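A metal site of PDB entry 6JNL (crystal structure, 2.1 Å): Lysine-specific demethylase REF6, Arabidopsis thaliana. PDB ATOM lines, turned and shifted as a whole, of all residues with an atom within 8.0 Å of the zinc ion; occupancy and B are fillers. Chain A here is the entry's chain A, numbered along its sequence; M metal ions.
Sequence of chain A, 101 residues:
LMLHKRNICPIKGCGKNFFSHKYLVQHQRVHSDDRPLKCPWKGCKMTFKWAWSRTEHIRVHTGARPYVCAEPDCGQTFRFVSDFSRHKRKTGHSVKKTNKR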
ATOM      1  N   VAL A  68      -7.369  19.473   0.125  1.00  0.00           N
ATOM      2  CA  VAL A  68      -6.241  18.504   0.210  1.00  0.00           C
ATOM      3  C   VAL A  68      -6.412  17.686   1.462  1.00  0.00           C
ATOM      4  O   VAL A  68      -6.327  18.232   2.546  1.00  0.00           O
ATOM      5  CB  VAL A  68      -4.881  19.238   0.244  1.00  0.00           C
ATOM      6  CG1 VAL A  68      -3.736  18.247   0.464  1.00  0.00           C
ATOM      7  CG2 VAL A  68      -4.683  20.005  -1.081  1.00  0.00           C
ATOM      8  N   CYS A  69      -6.686  16.381   1.329  1.00  0.00           N
ATOM      9  CA  CYS A  69      -6.739  15.483   2.495  1.00  0.00           C
ATOM     10  C   CYS A  69      -5.434  15.450   3.286  1.00  0.00           C
ATOM     11  O   CYS A  69      -4.369  15.226   2.712  1.00  0.00           O
ATOM     12  CB  CYS A  69      -7.018  14.068   2.081  1.00  0.00           C
ATOM     13  SG  CYS A  69      -7.406  13.204   3.577  1.00  0.00           S
ATOM     14  N   ALA A  70      -5.516  15.711   4.597  1.00  0.00           N
ATOM     15  CA  ALA A  70      -4.357  15.732   5.509  1.00  0.00           C
ATOM     16  C   ALA A  70      -3.955  14.341   6.097  1.00  0.00           C
ATOM     17  O   ALA A  70      -2.872  14.256   6.618  1.00  0.00           O
ATOM     18  CB  ALA A  70      -4.616  16.704   6.640  1.00  0.00           C
ATOM     19  N   GLU A  71      -4.799  13.300   6.019  1.00  0.00           N
ATOM     20  CA  GLU A  71      -4.459  11.954   6.558  1.00  0.00           C
ATOM     21  C   GLU A  71      -3.084  11.571   6.087  1.00  0.00           C
ATOM     22  O   GLU A  71      -2.758  11.794   4.898  1.00  0.00           O
ATOM     23  CB  GLU A  71      -5.458  10.854   6.156  1.00  0.00           C
ATOM     24  CG  GLU A  71      -5.236   9.483   6.829  1.00  0.00           C
ATOM     25  CD  GLU A  71      -5.725   9.394   8.280  1.00  0.00           C
ATOM     26  OE1 GLU A  71      -6.330  10.358   8.786  1.00  0.00           O
ATOM     27  OE2 GLU A  71      -5.494   8.336   8.914  1.00  0.00           O
ATOM     28  N   PRO A  72      -2.253  11.020   7.022  1.00  0.00           N
ATOM     29  CA  PRO A  72      -0.895  10.683   6.602  1.00  0.00           C
ATOM     30  C   PRO A  72      -0.919   9.725   5.386  1.00  0.00           C
ATOM     31  O   PRO A  72      -1.656   8.695   5.434  1.00  0.00           O
ATOM     32  CB  PRO A  72      -0.292  10.057   7.886  1.00  0.00           C
ATOM     33  CG  PRO A  72      -1.037  10.677   9.026  1.00  0.00           C
ATOM     34  CD  PRO A  72      -2.442  10.819   8.482  1.00  0.00           C
ATOM     35  N   ASP A  73      -0.228  10.098   4.297  1.00  0.00           N
ATOM     36  CA  ASP A  73      -0.119   9.214   3.127  1.00  0.00           C
ATOM     37  C   ASP A  73      -1.409   9.074   2.271  1.00  0.00           C
ATOM     38  O   ASP A  73      -1.363   8.346   1.269  1.00  0.00           O
ATOM     39  CB  ASP A  73       0.308   7.743   3.515  1.00  0.00           C
ATOM     40  CG  ASP A  73       1.612   7.669   4.323  1.00  0.00           C
ATOM     41  OD1 ASP A  73       2.611   8.224   3.849  1.00  0.00           O
ATOM     42  OD2 ASP A  73       1.634   7.001   5.407  1.00  0.00           O
ATOM     43  N   CYS A  74      -2.534   9.736   2.631  1.00  0.00           N
ATOM     44  CA  CYS A  74      -3.756   9.726   1.764  1.00  0.00           C
ATOM     45  C   CYS A  74      -3.516  10.328   0.369  1.00  0.00           C
ATOM     46  O   CYS A  74      -3.908   9.729  -0.635  1.00  0.00           O
ATOM     47  CB  CYS A  74      -4.985  10.414   2.390  1.00  0.00           C
ATOM     48  SG  CYS A  74      -6.387  10.525   1.238  1.00  0.00           S
ATOM     49  N   GLY A  75      -2.916  11.519   0.313  1.00  0.00           N
ATOM     50  CA  GLY A  75      -2.588  12.181  -0.956  1.00  0.00           C
ATOM     51  C   GLY A  75      -3.772  12.683  -1.847  1.00  0.00           C
ATOM     52  O   GLY A  75      -3.528  13.254  -2.933  1.00  0.00           O
ATOM     53  N   GLN A  76      -5.026  12.493  -1.431  1.00  0.00           N
ATOM     54  CA  GLN A  76      -6.127  12.882  -2.308  1.00  0.00           C
ATOM     55  C   GLN A  76      -6.510  14.369  -2.280  1.00  0.00           C
ATOM     56  O   GLN A  76      -6.380  15.042  -1.246  1.00  0.00           O
ATOM     57  CB  GLN A  76      -7.325  12.094  -1.970  1.00  0.00           C
ATOM     58  CG  GLN A  76      -7.174  10.704  -2.511  1.00  0.00           C
ATOM     59  CD  GLN A  76      -8.433   9.968  -2.316  1.00  0.00           C
ATOM     60  OE1 GLN A  76      -8.460   8.963  -1.673  1.00  0.00           O
ATOM     61  NE2 GLN A  76      -9.525  10.503  -2.844  1.00  0.00           N
ATOM     62  N   THR A  77      -6.951  14.870  -3.426  1.00  0.00           N
ATOM     63  CA  THR A  77      -7.334  16.278  -3.524  1.00  0.00           C
ATOM     64  C   THR A  77      -8.669  16.421  -4.215  1.00  0.00           C
ATOM     65  O   THR A  77      -9.088  15.526  -4.920  1.00  0.00           O
ATOM     66  CB  THR A  77      -6.275  17.134  -4.201  1.00  0.00           C
ATOM     67  OG1 THR A  77      -6.296  16.876  -5.604  1.00  0.00           O
ATOM     68  CG2 THR A  77      -4.942  16.834  -3.638  1.00  0.00           C
ATOM     69  N   PHE A  78      -9.366  17.521  -3.953  1.00  0.00           N
ATOM     70  CA  PHE A  78     -10.721  17.715  -4.494  1.00  0.00           C
ATOM     71  C   PHE A  78     -10.968  19.132  -5.022  1.00  0.00           C
ATOM     72  O   PHE A  78     -10.416  20.131  -4.515  1.00  0.00           O
ATOM     73  CB  PHE A  78     -11.743  17.343  -3.459  1.00  0.00           C
ATOM     74  CG  PHE A  78     -11.510  16.000  -2.890  1.00  0.00           C
ATOM     75  CD1 PHE A  78     -10.615  15.846  -1.848  1.00  0.00           C
ATOM     76  CD2 PHE A  78     -12.103  14.885  -3.463  1.00  0.00           C
ATOM     77  CE1 PHE A  78     -10.348  14.572  -1.338  1.00  0.00           C
ATOM     78  CE2 PHE A  78     -11.877  13.630  -2.954  1.00  0.00           C
ATOM     79  CZ  PHE A  78     -10.974  13.468  -1.899  1.00  0.00           C
ATOM     80  N   PHE A  84     -14.914  16.588  -0.853  1.00  0.00           N
ATOM     81  CA  PHE A  84     -13.974  16.491   0.229  1.00  0.00           C
ATOM     82  C   PHE A  84     -14.626  16.019   1.539  1.00  0.00           C
ATOM     83  O   PHE A  84     -14.083  15.135   2.230  1.00  0.00           O
ATOM     84  CB  PHE A  84     -13.253  17.774   0.371  1.00  0.00           C
ATOM     85  CG  PHE A  84     -12.229  17.792   1.469  1.00  0.00           C
ATOM     86  CD1 PHE A  84     -11.351  16.733   1.685  1.00  0.00           C
ATOM     87  CD2 PHE A  84     -12.096  18.951   2.285  1.00  0.00           C
ATOM     88  CE1 PHE A  84     -10.397  16.790   2.714  1.00  0.00           C
ATOM     89  CE2 PHE A  84     -11.114  19.032   3.279  1.00  0.00           C
ATOM     90  CZ  PHE A  84     -10.268  17.936   3.509  1.00  0.00           C
ATOM     91  N   HIS A  87     -15.584  12.257   1.239  1.00  0.00           N
ATOM     92  CA  HIS A  87     -14.410  11.415   1.461  1.00  0.00           C
ATOM     93  C   HIS A  87     -13.968  11.272   2.933  1.00  0.00           C
ATOM     94  O   HIS A  87     -13.587  10.206   3.371  1.00  0.00           O
ATOM     95  CB  HIS A  87     -13.283  11.894   0.598  1.00  0.00           C
ATOM     96  CG  HIS A  87     -11.914  11.464   1.056  1.00  0.00           C
ATOM     97  ND1 HIS A  87     -11.403  10.204   0.824  1.00  0.00           N
ATOM     98  CD2 HIS A  87     -10.920  12.167   1.643  1.00  0.00           C
ATOM     99  CE1 HIS A  87     -10.167  10.143   1.255  1.00  0.00           C
ATOM    100  NE2 HIS A  87      -9.855  11.323   1.768  1.00  0.00           N
ATOM    101  N   LYS A  88     -14.017  12.333   3.689  1.00  0.00           N
ATOM    102  CA  LYS A  88     -13.796  12.250   5.106  1.00  0.00           C
ATOM    103  C   LYS A  88     -14.841  11.364   5.826  1.00  0.00           C
ATOM    104  O   LYS A  88     -14.511  10.558   6.675  1.00  0.00           O
ATOM    105  CB  LYS A  88     -13.917  13.648   5.692  1.00  0.00           C
ATOM    106  CG  LYS A  88     -12.829  14.620   5.297  1.00  0.00           C
ATOM    107  CD  LYS A  88     -13.384  16.027   5.478  1.00  0.00           C
ATOM    108  CE  LYS A  88     -12.378  16.992   6.065  1.00  0.00           C
ATOM    109  NZ  LYS A  88     -13.082  18.285   6.232  1.00  0.00           N
ATOM    110  N   THR A  91     -14.203   7.752   4.792  1.00  0.00           N
ATOM    111  CA  THR A  91     -12.941   7.202   5.244  1.00  0.00           C
ATOM    112  C   THR A  91     -12.491   7.447   6.687  1.00  0.00           C
ATOM    113  O   THR A  91     -11.629   6.750   7.159  1.00  0.00           O
ATOM    114  CB  THR A  91     -11.778   7.723   4.358  1.00  0.00           C
ATOM    115  OG1 THR A  91     -11.513   9.126   4.610  1.00  0.00           O
ATOM    116  CG2 THR A  91     -12.083   7.451   2.894  1.00  0.00           C
ATOM    117  N   GLY A  92     -13.017   8.475   7.341  1.00  0.00           N
ATOM    118  CA  GLY A  92     -12.522   8.877   8.675  1.00  0.00           C
ATOM    119  C   GLY A  92     -11.317   9.803   8.781  1.00  0.00           C
ATOM    120  O   GLY A  92     -10.834  10.059   9.888  1.00  0.00           O
ATOM    121  N   HIS A  93     -10.843  10.352   7.660  1.00  0.00           N
ATOM    122  CA  HIS A  93      -9.666  11.263   7.656  1.00  0.00           C
ATOM    123  C   HIS A  93     -10.137  12.633   8.198  1.00  0.00           C
ATOM    124  O   HIS A  93     -11.264  13.009   7.920  1.00  0.00           O
ATOM    125  CB  HIS A  93      -9.106  11.329   6.244  1.00  0.00           C
ATOM    126  CG  HIS A  93      -8.764   9.988   5.671  1.00  0.00           C
ATOM    127  ND1 HIS A  93      -7.906   9.831   4.597  1.00  0.00           N
ATOM    128  CD2 HIS A  93      -9.119   8.737   6.028  1.00  0.00           C
ATOM    129  CE1 HIS A  93      -7.772   8.549   4.311  1.00  0.00           C
ATOM    130  NE2 HIS A  93      -8.505   7.868   5.165  1.00  0.00           N
ATOM    131  N   SER A  94      -9.335  13.335   9.017  1.00  0.00           N
ATOM    132  CA  SER A  94      -9.781  14.457   9.933  1.00  0.00           C
ATOM    133  C   SER A  94     -11.118  14.231  10.659  1.00  0.00           C
ATOM    134  O   SER A  94     -11.385  14.890  11.657  1.00  0.00           O
ATOM    135  CB  SER A  94      -9.822  15.819   9.218  1.00  0.00           C
ATOM    136  OG  SER A  94      -8.850  15.874   8.186  1.00  0.00           O
HETATM  137 ZN    ZN M   1      -7.973  11.122   2.828  1.00  0.00          ZN
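N of Gln 76 lies close to SG of Cys 74.
A ring nitrogen (NE2) of His 93 sits close to the side-chain hydroxyl of Thr 91 (3.3 Å).
OG1 of Thr 91 lies within hydrogen-bond range of O of His 87.
SG of Cys 69 lies close to N of Glu 71, 3.6 Å away.
The backbone carbonyl oxygen of Gln 76 is in hydrogen-bond range of the backbone NH of Cys 69 (2.9 Å).
Four residues have an atom within 4 Å of the zinc ion: Cys 69, Cys 74, His 87 and His 93.
The nearest printed residue that does not touch the zinc ion is Glu 71 (4.2 Å).
The zinc ion is bound by a ring nitrogen (NE2) of His 87 (2.2 Å), a ring nitrogen (ND1) of His 93 (2.2 Å), the side-chain sulfur of Cys 69 (2.3 Å) and the side-chain sulfur of Cys 74 (2.3 Å).
The zinc ion has four donor atoms within binding distance.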
